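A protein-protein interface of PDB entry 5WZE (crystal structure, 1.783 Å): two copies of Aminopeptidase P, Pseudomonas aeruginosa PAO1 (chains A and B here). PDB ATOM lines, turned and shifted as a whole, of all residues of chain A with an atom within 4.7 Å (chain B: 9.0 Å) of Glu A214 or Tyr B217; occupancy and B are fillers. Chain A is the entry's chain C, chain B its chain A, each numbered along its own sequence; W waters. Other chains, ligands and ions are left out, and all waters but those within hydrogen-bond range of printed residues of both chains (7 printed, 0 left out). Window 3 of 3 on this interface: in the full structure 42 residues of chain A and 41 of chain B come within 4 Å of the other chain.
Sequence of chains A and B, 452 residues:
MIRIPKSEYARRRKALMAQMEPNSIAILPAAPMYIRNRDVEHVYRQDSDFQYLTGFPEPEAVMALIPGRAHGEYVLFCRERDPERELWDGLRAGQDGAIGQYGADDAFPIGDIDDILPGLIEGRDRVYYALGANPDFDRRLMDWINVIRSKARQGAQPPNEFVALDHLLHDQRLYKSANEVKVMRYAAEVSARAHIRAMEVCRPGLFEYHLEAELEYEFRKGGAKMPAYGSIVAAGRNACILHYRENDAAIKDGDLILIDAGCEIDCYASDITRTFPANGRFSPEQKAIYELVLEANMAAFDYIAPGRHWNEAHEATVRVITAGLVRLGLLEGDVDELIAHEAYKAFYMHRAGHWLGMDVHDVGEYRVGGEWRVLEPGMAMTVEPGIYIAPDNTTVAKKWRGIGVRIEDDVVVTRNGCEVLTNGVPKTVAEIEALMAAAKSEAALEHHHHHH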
ATOM      1  N   ARG A 197      -9.606  -8.479 -13.408  1.00  0.00           N
ATOM      2  CA  ARG A 197      -8.586  -8.053 -12.462  1.00  0.00           C
ATOM      3  C   ARG A 197      -9.201  -7.552 -11.169  1.00  0.00           C
ATOM      4  O   ARG A 197      -8.726  -7.883 -10.083  1.00  0.00           O
ATOM      5  CB  ARG A 197      -7.717  -6.963 -13.082  1.00  0.00           C
ATOM      6  CG  ARG A 197      -6.711  -7.450 -14.071  1.00  0.00           C
ATOM      7  CD  ARG A 197      -5.398  -7.701 -13.359  1.00  0.00           C
ATOM      8  NE  ARG A 197      -5.454  -8.905 -12.563  1.00  0.00           N
ATOM      9  CZ  ARG A 197      -4.788  -9.103 -11.433  1.00  0.00           C
ATOM     10  NH1 ARG A 197      -4.923 -10.252 -10.811  1.00  0.00           N
ATOM     11  NH2 ARG A 197      -4.005  -8.170 -10.915  1.00  0.00           N
ATOM     12  N   ALA A 198     -10.238  -6.725 -11.268  1.00  0.00           N
ATOM     13  CA  ALA A 198     -10.913  -6.245 -10.069  1.00  0.00           C
ATOM     14  C   ALA A 198     -11.408  -7.399  -9.213  1.00  0.00           C
ATOM     15  O   ALA A 198     -11.293  -7.360  -7.989  1.00  0.00           O
ATOM     16  CB  ALA A 198     -12.075  -5.325 -10.441  1.00  0.00           C
ATOM     17  N   VAL A 201      -8.338  -9.162  -7.407  1.00  0.00           N
ATOM     18  CA  VAL A 201      -7.611  -8.410  -6.395  1.00  0.00           C
ATOM     19  C   VAL A 201      -8.464  -8.129  -5.183  1.00  0.00           C
ATOM     20  O   VAL A 201      -7.947  -7.906  -4.086  1.00  0.00           O
ATOM     21  CB  VAL A 201      -7.051  -7.121  -7.019  1.00  0.00           C
ATOM     22  CG1 VAL A 201      -6.371  -6.242  -6.025  1.00  0.00           C
ATOM     23  CG2 VAL A 201      -6.094  -7.452  -8.164  1.00  0.00           C
ATOM     24  N   HIS A 210      -9.279   1.153  -4.581  1.00  0.00           N
ATOM     25  CA  HIS A 210      -8.305   0.143  -4.985  1.00  0.00           C
ATOM     26  C   HIS A 210      -8.797  -0.629  -6.204  1.00  0.00           C
ATOM     27  O   HIS A 210      -8.028  -0.895  -7.134  1.00  0.00           O
ATOM     28  CB  HIS A 210      -7.995  -0.804  -3.828  1.00  0.00           C
ATOM     29  CG  HIS A 210      -7.178  -0.175  -2.751  1.00  0.00           C
ATOM     30  ND1 HIS A 210      -7.679   0.092  -1.499  1.00  0.00           N
ATOM     31  CD2 HIS A 210      -5.900   0.275  -2.750  1.00  0.00           C
ATOM     32  CE1 HIS A 210      -6.743   0.663  -0.765  1.00  0.00           C
ATOM     33  NE2 HIS A 210      -5.656   0.795  -1.503  1.00  0.00           N
ATOM     34  N   LEU A 211     -10.090  -0.948  -6.245  1.00  0.00           N
ATOM     35  CA  LEU A 211     -10.615  -1.659  -7.405  1.00  0.00           C
ATOM     36  C   LEU A 211     -10.732  -0.738  -8.615  1.00  0.00           C
ATOM     37  O   LEU A 211     -10.477  -1.163  -9.743  1.00  0.00           O
ATOM     38  CB  LEU A 211     -11.969  -2.277  -7.079  1.00  0.00           C
ATOM     39  CG  LEU A 211     -12.020  -3.141  -5.826  1.00  0.00           C
ATOM     40  CD1 LEU A 211     -13.353  -3.861  -5.769  1.00  0.00           C
ATOM     41  CD2 LEU A 211     -10.894  -4.129  -5.791  1.00  0.00           C
ATOM     42  N   GLU A 212     -11.123   0.520  -8.403  1.00  0.00           N
ATOM     43  CA  GLU A 212     -11.128   1.456  -9.522  1.00  0.00           C
ATOM     44  C   GLU A 212      -9.733   1.583 -10.125  1.00  0.00           C
ATOM     45  O   GLU A 212      -9.599   1.692 -11.342  1.00  0.00           O
ATOM     46  CB  GLU A 212     -11.653   2.830  -9.098  1.00  0.00           C
ATOM     47  CG  GLU A 212     -11.888   3.752 -10.299  1.00  0.00           C
ATOM     48  CD  GLU A 212     -12.415   5.141  -9.961  1.00  0.00           C
ATOM     49  OE1 GLU A 212     -12.481   5.508  -8.778  1.00  0.00           O
ATOM     50  OE2 GLU A 212     -12.755   5.869 -10.911  1.00  0.00           O
ATOM     51  N   ALA A 213      -8.696   1.499  -9.288  1.00  0.00           N
ATOM     52  CA  ALA A 213      -7.319   1.528  -9.768  1.00  0.00           C
ATOM     53  C   ALA A 213      -7.051   0.413 -10.764  1.00  0.00           C
ATOM     54  O   ALA A 213      -6.461   0.643 -11.820  1.00  0.00           O
ATOM     55  CB  ALA A 213      -6.353   1.424  -8.595  1.00  0.00           C
ATOM     56  N   GLU A 214      -7.466  -0.811 -10.435  1.00  0.00           N
ATOM     57  CA  GLU A 214      -7.258  -1.918 -11.357  1.00  0.00           C
ATOM     58  C   GLU A 214      -7.982  -1.677 -12.666  1.00  0.00           C
ATOM     59  O   GLU A 214      -7.462  -1.999 -13.733  1.00  0.00           O
ATOM     60  CB  GLU A 214      -7.718  -3.230 -10.734  1.00  0.00           C
ATOM     61  CG  GLU A 214      -7.044  -3.550  -9.423  1.00  0.00           C
ATOM     62  CD  GLU A 214      -5.557  -3.834  -9.576  1.00  0.00           C
ATOM     63  OE1 GLU A 214      -5.147  -4.277 -10.657  1.00  0.00           O
ATOM     64  OE2 GLU A 214      -4.813  -3.617  -8.611  1.00  0.00           O
ATOM     65  N   LEU A 215      -9.186  -1.118 -12.605  1.00  0.00           N
ATOM     66  CA  LEU A 215      -9.915  -0.856 -13.837  1.00  0.00           C
ATOM     67  C   LEU A 215      -9.144   0.119 -14.721  1.00  0.00           C
ATOM     68  O   LEU A 215      -8.846  -0.186 -15.876  1.00  0.00           O
ATOM     69  CB  LEU A 215     -11.316  -0.324 -13.532  1.00  0.00           C
ATOM     70  CG  LEU A 215     -12.260  -1.242 -12.753  1.00  0.00           C
ATOM     71  CD1 LEU A 215     -13.537  -0.526 -12.342  1.00  0.00           C
ATOM     72  CD2 LEU A 215     -12.584  -2.513 -13.535  1.00  0.00           C
ATOM     73  N   GLU A 216      -8.788   1.289 -14.179  1.00  0.00           N
ATOM     74  CA  GLU A 216      -8.109   2.295 -14.989  1.00  0.00           C
ATOM     75  C   GLU A 216      -6.790   1.758 -15.530  1.00  0.00           C
ATOM     76  O   GLU A 216      -6.445   2.001 -16.689  1.00  0.00           O
ATOM     77  CB  GLU A 216      -7.881   3.568 -14.174  1.00  0.00           C
ATOM     78  CG  GLU A 216      -9.129   4.387 -13.924  1.00  0.00           C
ATOM     79  CD  GLU A 216      -9.474   5.341 -15.070  1.00  0.00           C
ATOM     80  OE1 GLU A 216      -8.602   5.628 -15.924  1.00  0.00           O
ATOM     81  OE2 GLU A 216     -10.625   5.812 -15.106  1.00  0.00           O
ATOM     82  N   TYR A 217      -6.055   1.009 -14.708  1.00  0.00           N
ATOM     83  CA  TYR A 217      -4.801   0.405 -15.137  1.00  0.00           C
ATOM     84  C   TYR A 217      -4.995  -0.425 -16.396  1.00  0.00           C
ATOM     85  O   TYR A 217      -4.289  -0.243 -17.388  1.00  0.00           O
ATOM     86  CB  TYR A 217      -4.247  -0.447 -13.999  1.00  0.00           C
ATOM     87  CG  TYR A 217      -2.867  -1.037 -14.208  1.00  0.00           C
ATOM     88  CD1 TYR A 217      -1.862  -0.320 -14.832  1.00  0.00           C
ATOM     89  CD2 TYR A 217      -2.560  -2.303 -13.724  1.00  0.00           C
ATOM     90  CE1 TYR A 217      -0.611  -0.857 -14.997  1.00  0.00           C
ATOM     91  CE2 TYR A 217      -1.308  -2.843 -13.883  1.00  0.00           C
ATOM     92  CZ  TYR A 217      -0.337  -2.113 -14.517  1.00  0.00           C
ATOM     93  OH  TYR A 217       0.916  -2.644 -14.677  1.00  0.00           O
ATOM     94  N   GLU A 218      -5.970  -1.334 -16.380  1.00  0.00           N
ATOM     95  CA  GLU A 218      -6.168  -2.217 -17.524  1.00  0.00           C
ATOM     96  C   GLU A 218      -6.723  -1.459 -18.731  1.00  0.00           C
ATOM     97  O   GLU A 218      -6.285  -1.690 -19.862  1.00  0.00           O
ATOM     98  CB  GLU A 218      -7.092  -3.356 -17.122  1.00  0.00           C
ATOM     99  CG  GLU A 218      -7.158  -4.470 -18.110  1.00  0.00           C
ATOM    100  CD  GLU A 218      -5.881  -5.298 -18.156  1.00  0.00           C
ATOM    101  OE1 GLU A 218      -5.254  -5.538 -17.104  1.00  0.00           O
ATOM    102  OE2 GLU A 218      -5.523  -5.713 -19.267  1.00  0.00           O
ATOM    103  N   VAL B 190       3.133   9.518  -2.848  1.00  0.00           N
ATOM    104  CA  VAL B 190       2.408   8.686  -3.797  1.00  0.00           C
ATOM    105  C   VAL B 190       2.972   8.872  -5.198  1.00  0.00           C
ATOM    106  O   VAL B 190       3.221   7.903  -5.917  1.00  0.00           O
ATOM    107  CB  VAL B 190       0.908   8.997  -3.752  1.00  0.00           C
ATOM    108  CG1 VAL B 190       0.218   8.279  -4.870  1.00  0.00           C
ATOM    109  CG2 VAL B 190       0.337   8.580  -2.408  1.00  0.00           C
ATOM    110  N   ARG B 193       6.242   7.047  -5.763  1.00  0.00           N
ATOM    111  CA  ARG B 193       6.129   5.621  -6.053  1.00  0.00           C
ATOM    112  C   ARG B 193       5.687   5.394  -7.487  1.00  0.00           C
ATOM    113  O   ARG B 193       6.133   4.447  -8.136  1.00  0.00           O
ATOM    114  CB  ARG B 193       5.159   4.946  -5.088  1.00  0.00           C
ATOM    115  CG  ARG B 193       5.764   4.638  -3.731  1.00  0.00           C
ATOM    116  CD  ARG B 193       4.914   3.649  -2.943  1.00  0.00           C
ATOM    117  NE  ARG B 193       3.556   4.140  -2.815  1.00  0.00           N
ATOM    118  CZ  ARG B 193       3.116   4.863  -1.795  1.00  0.00           C
ATOM    119  NH1 ARG B 193       3.928   5.172  -0.796  1.00  0.00           N
ATOM    120  NH2 ARG B 193       1.855   5.269  -1.775  1.00  0.00           N
ATOM    121  N   ALA B 194       4.815   6.265  -8.002  1.00  0.00           N
ATOM    122  CA  ALA B 194       4.341   6.108  -9.370  1.00  0.00           C
ATOM    123  C   ALA B 194       5.477   6.291 -10.365  1.00  0.00           C
ATOM    124  O   ALA B 194       5.579   5.550 -11.345  1.00  0.00           O
ATOM    125  CB  ALA B 194       3.218   7.101  -9.659  1.00  0.00           C
ATOM    126  N   ARG B 197       7.645   3.201 -10.465  1.00  0.00           N
ATOM    127  CA  ARG B 197       7.041   2.107 -11.221  1.00  0.00           C
ATOM    128  C   ARG B 197       7.163   2.333 -12.725  1.00  0.00           C
ATOM    129  O   ARG B 197       7.447   1.394 -13.473  1.00  0.00           O
ATOM    130  CB  ARG B 197       5.578   1.906 -10.809  1.00  0.00           C
ATOM    131  CG  ARG B 197       5.410   1.261  -9.439  1.00  0.00           C
ATOM    132  CD  ARG B 197       6.094  -0.120  -9.391  1.00  0.00           C
ATOM    133  NE  ARG B 197       5.392  -1.094 -10.217  1.00  0.00           N
ATOM    134  CZ  ARG B 197       5.974  -2.081 -10.889  1.00  0.00           C
ATOM    135  NH1 ARG B 197       7.291  -2.234 -10.866  1.00  0.00           N
ATOM    136  NH2 ARG B 197       5.227  -2.914 -11.598  1.00  0.00           N
ATOM    137  N   VAL B 201       9.006  -0.450 -15.169  1.00  0.00           N
ATOM    138  CA  VAL B 201       8.280  -1.145 -16.218  1.00  0.00           C
ATOM    139  C   VAL B 201       8.793  -0.811 -17.613  1.00  0.00           C
ATOM    140  O   VAL B 201       8.591  -1.600 -18.542  1.00  0.00           O
ATOM    141  CB  VAL B 201       6.786  -0.809 -16.061  1.00  0.00           C
ATOM    142  CG1 VAL B 201       5.948  -1.389 -17.169  1.00  0.00           C
ATOM    143  CG2 VAL B 201       6.288  -1.297 -14.718  1.00  0.00           C
ATOM    144  N   TYR B 209       1.710   5.371 -23.464  1.00  0.00           N
ATOM    145  CA  TYR B 209       0.536   5.230 -22.604  1.00  0.00           C
ATOM    146  C   TYR B 209       0.672   4.071 -21.625  1.00  0.00           C
ATOM    147  O   TYR B 209       0.041   4.089 -20.568  1.00  0.00           O
ATOM    148  CB  TYR B 209      -0.740   5.083 -23.433  1.00  0.00           C
ATOM    149  CG  TYR B 209      -0.809   3.904 -24.359  1.00  0.00           C
ATOM    150  CD1 TYR B 209      -1.028   2.627 -23.883  1.00  0.00           C
ATOM    151  CD2 TYR B 209      -0.699   4.078 -25.724  1.00  0.00           C
ATOM    152  CE1 TYR B 209      -1.107   1.551 -24.742  1.00  0.00           C
ATOM    153  CE2 TYR B 209      -0.772   3.022 -26.584  1.00  0.00           C
ATOM    154  CZ  TYR B 209      -0.979   1.763 -26.095  1.00  0.00           C
ATOM    155  OH  TYR B 209      -1.052   0.728 -26.972  1.00  0.00           O
ATOM    156  N   HIS B 210       1.476   3.057 -21.950  1.00  0.00           N
ATOM    157  CA  HIS B 210       1.756   2.023 -20.959  1.00  0.00           C
ATOM    158  C   HIS B 210       2.386   2.622 -19.710  1.00  0.00           C
ATOM    159  O   HIS B 210       2.090   2.202 -18.590  1.00  0.00           O
ATOM    160  CB  HIS B 210       2.668   0.944 -21.535  1.00  0.00           C
ATOM    161  CG  HIS B 210       2.018   0.074 -22.557  1.00  0.00           C
ATOM    162  ND1 HIS B 210       2.319   0.154 -23.895  1.00  0.00           N
ATOM    163  CD2 HIS B 210       1.097  -0.909 -22.437  1.00  0.00           C
ATOM    164  CE1 HIS B 210       1.607  -0.736 -24.560  1.00  0.00           C
ATOM    165  NE2 HIS B 210       0.859  -1.396 -23.698  1.00  0.00           N
ATOM    166  N   LEU B 211       3.246   3.622 -19.874  1.00  0.00           N
ATOM    167  CA  LEU B 211       3.817   4.243 -18.690  1.00  0.00           C
ATOM    168  C   LEU B 211       2.793   5.126 -17.982  1.00  0.00           C
ATOM    169  O   LEU B 211       2.760   5.183 -16.748  1.00  0.00           O
ATOM    170  CB  LEU B 211       5.065   5.026 -19.066  1.00  0.00           C
ATOM    171  CG  LEU B 211       6.108   4.227 -19.843  1.00  0.00           C
ATOM    172  CD1 LEU B 211       7.379   5.041 -20.002  1.00  0.00           C
ATOM    173  CD2 LEU B 211       6.397   2.903 -19.174  1.00  0.00           C
ATOM    174  N   GLU B 212       1.935   5.809 -18.740  1.00  0.00           N
ATOM    175  CA  GLU B 212       0.868   6.578 -18.111  1.00  0.00           C
ATOM    176  C   GLU B 212      -0.065   5.663 -17.340  1.00  0.00           C
ATOM    177  O   GLU B 212      -0.607   6.049 -16.303  1.00  0.00           O
ATOM    178  CB  GLU B 212       0.085   7.380 -19.152  1.00  0.00           C
ATOM    179  CG  GLU B 212      -0.848   8.398 -18.515  1.00  0.00           C
ATOM    180  CD  GLU B 212      -1.673   9.217 -19.497  1.00  0.00           C
ATOM    181  OE1 GLU B 212      -1.654   8.944 -20.703  1.00  0.00           O
ATOM    182  OE2 GLU B 212      -2.350  10.147 -19.030  1.00  0.00           O
ATOM    183  N   ALA B 213      -0.255   4.441 -17.831  1.00  0.00           N
ATOM    184  CA  ALA B 213      -1.071   3.478 -17.099  1.00  0.00           C
ATOM    185  C   ALA B 213      -0.481   3.199 -15.729  1.00  0.00           C
ATOM    186  O   ALA B 213      -1.206   3.151 -14.732  1.00  0.00           O
ATOM    187  CB  ALA B 213      -1.207   2.179 -17.887  1.00  0.00           C
ATOM    188  N   GLU B 214       0.837   3.020 -15.657  1.00  0.00           N
ATOM    189  CA  GLU B 214       1.452   2.768 -14.362  1.00  0.00           C
ATOM    190  C   GLU B 214       1.248   3.953 -13.432  1.00  0.00           C
ATOM    191  O   GLU B 214       0.993   3.776 -12.238  1.00  0.00           O
ATOM    192  CB  GLU B 214       2.943   2.465 -14.525  1.00  0.00           C
ATOM    193  CG  GLU B 214       3.258   1.249 -15.363  1.00  0.00           C
ATOM    194  CD  GLU B 214       2.860  -0.063 -14.703  1.00  0.00           C
ATOM    195  OE1 GLU B 214       2.523  -0.997 -15.446  1.00  0.00           O
ATOM    196  OE2 GLU B 214       2.884  -0.150 -13.462  1.00  0.00           O
ATOM    197  N   LEU B 215       1.341   5.173 -13.968  1.00  0.00           N
ATOM    198  CA  LEU B 215       1.188   6.361 -13.142  1.00  0.00           C
ATOM    199  C   LEU B 215      -0.217   6.435 -12.562  1.00  0.00           C
ATOM    200  O   LEU B 215      -0.395   6.576 -11.352  1.00  0.00           O
ATOM    201  CB  LEU B 215       1.497   7.619 -13.963  1.00  0.00           C
ATOM    202  CG  LEU B 215       2.897   7.771 -14.551  1.00  0.00           C
ATOM    203  CD1 LEU B 215       2.979   8.998 -15.460  1.00  0.00           C
ATOM    204  CD2 LEU B 215       3.888   7.863 -13.430  1.00  0.00           C
ATOM    205  N   GLU B 216      -1.228   6.350 -13.422  1.00  0.00           N
ATOM    206  CA  GLU B 216      -2.601   6.388 -12.941  1.00  0.00           C
ATOM    207  C   GLU B 216      -2.865   5.264 -11.937  1.00  0.00           C
ATOM    208  O   GLU B 216      -3.473   5.492 -10.890  1.00  0.00           O
ATOM    209  CB  GLU B 216      -3.560   6.330 -14.130  1.00  0.00           C
ATOM    210  CG  GLU B 216      -3.551   7.593 -14.995  1.00  0.00           C
ATOM    211  CD  GLU B 216      -4.454   8.705 -14.446  1.00  0.00           C
ATOM    212  OE1 GLU B 216      -5.270   8.427 -13.543  1.00  0.00           O
ATOM    213  OE2 GLU B 216      -4.358   9.854 -14.924  1.00  0.00           O
ATOM    214  N   TYR B 217      -2.371   4.058 -12.224  1.00  0.00           N
ATOM    215  CA  TYR B 217      -2.528   2.925 -11.312  1.00  0.00           C
ATOM    216  C   TYR B 217      -2.057   3.266  -9.903  1.00  0.00           C
ATOM    217  O   TYR B 217      -2.811   3.136  -8.934  1.00  0.00           O
ATOM    218  CB  TYR B 217      -1.756   1.727 -11.857  1.00  0.00           C
ATOM    219  CG  TYR B 217      -1.954   0.423 -11.114  1.00  0.00           C
ATOM    220  CD1 TYR B 217      -3.199   0.034 -10.654  1.00  0.00           C
ATOM    221  CD2 TYR B 217      -0.892  -0.440 -10.923  1.00  0.00           C
ATOM    222  CE1 TYR B 217      -3.371  -1.176 -10.007  1.00  0.00           C
ATOM    223  CE2 TYR B 217      -1.052  -1.644 -10.279  1.00  0.00           C
ATOM    224  CZ  TYR B 217      -2.281  -2.009  -9.822  1.00  0.00           C
ATOM    225  OH  TYR B 217      -2.399  -3.216  -9.181  1.00  0.00           O
ATOM    226  N   GLU B 218      -0.815   3.731  -9.778  1.00  0.00           N
ATOM    227  CA  GLU B 218      -0.248   4.031  -8.472  1.00  0.00           C
ATOM    228  C   GLU B 218      -0.921   5.238  -7.835  1.00  0.00           C
ATOM    229  O   GLU B 218      -1.135   5.265  -6.619  1.00  0.00           O
ATOM    230  CB  GLU B 218       1.251   4.266  -8.612  1.00  0.00           C
ATOM    231  CG  GLU B 218       2.004   4.255  -7.325  1.00  0.00           C
ATOM    232  CD  GLU B 218       2.034   2.878  -6.669  1.00  0.00           C
ATOM    233  OE1 GLU B 218       2.062   1.857  -7.389  1.00  0.00           O
ATOM    234  OE2 GLU B 218       2.023   2.837  -5.428  1.00  0.00           O
ATOM    235  N   PHE B 219      -1.232   6.255  -8.642  1.00  0.00           N
ATOM    236  CA  PHE B 219      -2.014   7.389  -8.158  1.00  0.00           C
ATOM    237  C   PHE B 219      -3.296   6.905  -7.478  1.00  0.00           C
ATOM    238  O   PHE B 219      -3.564   7.231  -6.320  1.00  0.00           O
ATOM    239  CB  PHE B 219      -2.367   8.329  -9.317  1.00  0.00           C
ATOM    240  CG  PHE B 219      -1.203   9.137  -9.880  1.00  0.00           C
ATOM    241  CD1 PHE B 219       0.041   9.139  -9.288  1.00  0.00           C
ATOM    242  CD2 PHE B 219      -1.398   9.932 -11.005  1.00  0.00           C
ATOM    243  CE1 PHE B 219       1.088   9.906  -9.827  1.00  0.00           C
ATOM    244  CE2 PHE B 219      -0.366  10.696 -11.547  1.00  0.00           C
ATOM    245  CZ  PHE B 219       0.872  10.683 -10.955  1.00  0.00           C
ATOM    246  N   ARG B 220      -4.081   6.100  -8.186  1.00  0.00           N
ATOM    247  CA  ARG B 220      -5.396   5.720  -7.686  1.00  0.00           C
ATOM    248  C   ARG B 220      -5.295   4.776  -6.496  1.00  0.00           C
ATOM    249  O   ARG B 220      -6.092   4.872  -5.557  1.00  0.00           O
ATOM    250  CB  ARG B 220      -6.206   5.114  -8.820  1.00  0.00           C
ATOM    251  CG  ARG B 220      -6.293   6.070  -9.987  1.00  0.00           C
ATOM    252  CD  ARG B 220      -7.455   5.853 -10.900  1.00  0.00           C
ATOM    253  NE  ARG B 220      -7.497   6.854 -11.965  1.00  0.00           N
ATOM    254  CZ  ARG B 220      -8.477   7.746 -12.103  1.00  0.00           C
ATOM    255  NH1 ARG B 220      -9.493   7.748 -11.251  1.00  0.00           N
ATOM    256  NH2 ARG B 220      -8.446   8.636 -13.091  1.00  0.00           N
ATOM    257  N   LYS B 221      -4.310   3.885  -6.500  1.00  0.00           N
ATOM    258  CA  LYS B 221      -4.098   3.035  -5.343  1.00  0.00           C
ATOM    259  C   LYS B 221      -3.776   3.854  -4.108  1.00  0.00           C
ATOM    260  O   LYS B 221      -4.070   3.422  -2.988  1.00  0.00           O
ATOM    261  CB  LYS B 221      -2.995   2.023  -5.633  1.00  0.00           C
ATOM    262  CG  LYS B 221      -3.488   0.800  -6.391  1.00  0.00           C
ATOM    263  CD  LYS B 221      -2.368   0.005  -7.036  1.00  0.00           C
ATOM    264  CE  LYS B 221      -1.117  -0.092  -6.204  1.00  0.00           C
ATOM    265  NZ  LYS B 221      -0.064  -0.826  -6.957  1.00  0.00           N
ATOM    266  N   GLY B 222      -3.192   5.034  -4.283  1.00  0.00           N
ATOM    267  CA  GLY B 222      -2.944   5.901  -3.149  1.00  0.00           C
ATOM    268  C   GLY B 222      -4.106   6.761  -2.711  1.00  0.00           C
ATOM    269  O   GLY B 222      -3.969   7.530  -1.761  1.00  0.00           O
ATOM    270  N   GLY B 223      -5.250   6.658  -3.371  1.00  0.00           N
ATOM    271  CA  GLY B 223      -6.413   7.424  -2.992  1.00  0.00           C
ATOM    272  C   GLY B 223      -6.697   8.657  -3.830  1.00  0.00           C
ATOM    273  O   GLY B 223      -7.643   9.379  -3.523  1.00  0.00           O
ATOM    274  N   ALA B 224      -5.916   8.923  -4.872  1.00  0.00           N
ATOM    275  CA  ALA B 224      -6.130  10.124  -5.670  1.00  0.00           C
ATOM    276  C   ALA B 224      -7.382   9.976  -6.522  1.00  0.00           C
ATOM    277  O   ALA B 224      -7.572   8.957  -7.184  1.00  0.00           O
ATOM    278  CB  ALA B 224      -4.919  10.391  -6.554  1.00  0.00           C
ATOM    279  N   PRO B 227      -5.378  13.079 -11.297  1.00  0.00           N
ATOM    280  CA  PRO B 227      -4.052  13.697 -11.261  1.00  0.00           C
ATOM    281  C   PRO B 227      -4.163  15.184 -10.972  1.00  0.00           C
ATOM    282  O   PRO B 227      -5.209  15.809 -11.156  1.00  0.00           O
ATOM    283  CB  PRO B 227      -3.495  13.463 -12.667  1.00  0.00           C
ATOM    284  CG  PRO B 227      -4.491  12.651 -13.386  1.00  0.00           C
ATOM    285  CD  PRO B 227      -5.781  12.718 -12.657  1.00  0.00           C
ATOM    286  N   SER B 231      -0.982  13.870 -17.218  1.00  0.00           N
ATOM    287  CA  SER B 231       0.386  13.377 -17.222  1.00  0.00           C
ATOM    288  C   SER B 231       1.042  13.569 -18.581  1.00  0.00           C
ATOM    289  O   SER B 231       0.434  13.326 -19.621  1.00  0.00           O
ATOM    290  CB  SER B 231       0.428  11.898 -16.860  1.00  0.00           C
ATOM    291  OG  SER B 231       0.003  11.682 -15.538  1.00  0.00           O
ATOM    292  N   CYS B 263       0.014  13.221  -8.686  1.00  0.00           N
ATOM    293  CA  CYS B 263      -1.342  13.075  -8.185  1.00  0.00           C
ATOM    294  C   CYS B 263      -1.732  14.296  -7.362  1.00  0.00           C
ATOM    295  O   CYS B 263      -0.891  15.097  -6.958  1.00  0.00           O
ATOM    296  CB  CYS B 263      -1.464  11.817  -7.323  1.00  0.00           C
ATOM    297  SG  CYS B 263      -0.786  11.969  -5.679  1.00  0.00           S
HETATM  298  O   HOH W   1       2.402  -2.503 -12.159  1.00  0.00           O
HETATM  299  O   HOH W   2       3.796  -3.882 -15.977  1.00  0.00           O
HETATM  300  O   HOH W   3      -2.648  -5.590  -7.258  1.00  0.00           O
HETATM  301  O   HOH W   4     -12.211   8.517 -11.580  1.00  0.00           O
HETATM  302  O   HOH W   5      -2.747  -5.393 -11.386  1.00  0.00           O
HETATM  303  O   HOH W   6     -10.605   8.624 -15.603  1.00  0.00           O
HETATM  304  O   HOH W   7      -9.667   5.930  -8.869  1.00  0.00           O
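Water W4 lies within hydrogen-bond range of OE2 of Glu A212 (2.8 Å) and NH1 of Arg B220 (2.8 Å). Water W6 bridges the side-chain carboxylate (OE2) of Glu A216 (2.9 Å) and the guanidinium group (NH2) of Arg B220 (3.3 Å).
Of the 24 printed residues of chain B, 5 touch a printed residue of chain A. Printed residues of chain B that touch a printed residue of chain A: Ala B213, Glu B214, Tyr B217, Arg B220 and Lys B221. Hydrophobic or aromatic side chains of chain B that line the printed part of chain A: Ala B213 and Tyr B217. Hydrophobic or aromatic side chains of chain A within 4 Å of the printed part of chain B: His A210, Ala A213 and Tyr A217. Along chain A the printed residues that touch a printed residue of chain B span positions 210 to 217. Among the printed residues, Asp or Glu carboxylates within 4 Å of a Lys or Arg side-chain nitrogen of the other chain: Glu A212 with Arg B220 (3.8 Å).
The side-chain carboxylate (OE1) of Glu B216 is in salt-bridge range of the guanidinium group (NE) of Arg B220 (3.2 Å). The side-chain carboxylate of Glu B218 lies within salt-bridge range of the side-chain amino group of Lys B221 (3.5 Å).
Of chain B, only Tyr B217 (3.5 Å), Arg B220 (3.7 Å) and Lys B221 (3.7 Å) come within 4 Å of Ala A213. Glu A214 touches one residue of chain B. Printed residues of chain B within 4 Å of Tyr A217: Ala B213, Glu B214 and Tyr B217. Printed residues of chain A within 4 Å of Glu B214: Tyr A217 (2.4 Å). Printed residues of chain A within 4 Å of Lys B221: His A210 and Ala A213. The nearest residue of chain B that does not touch Glu A214 is Lys B221 (4.6 Å). The nearest printed residue of chain A that does not touch Tyr B217 is His A210 (5.5 Å). The nearest printed residue of chain A that does not touch Lys B221 is Glu A214 (4.6 Å).
The guanidinium group of Arg B220 is in salt-bridge range of the side-chain carboxylate of Glu A212. The side-chain hydroxyl (OH) of Tyr B217 is in hydrogen-bond range of the side-chain carboxylate (OE2) of Glu A214 (2.5 Å). The side-chain hydroxyl (OH) of Tyr A217 sits at hydrogen-bond distance from the side-chain carboxylate (OE1) of Glu B214 (2.4 Å). The backbone carbonyl oxygen (O) of Lys B221 sits at hydrogen-bond distance from a ring nitrogen (NE2) of His A210 (3.4 Å).
Glu A214 touches Tyr B217, and with the chains exchanged Tyr A217 touches Glu B214. Tyr B217 touches its own counterpart, Tyr A217. 11 positions are printed for both chains.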
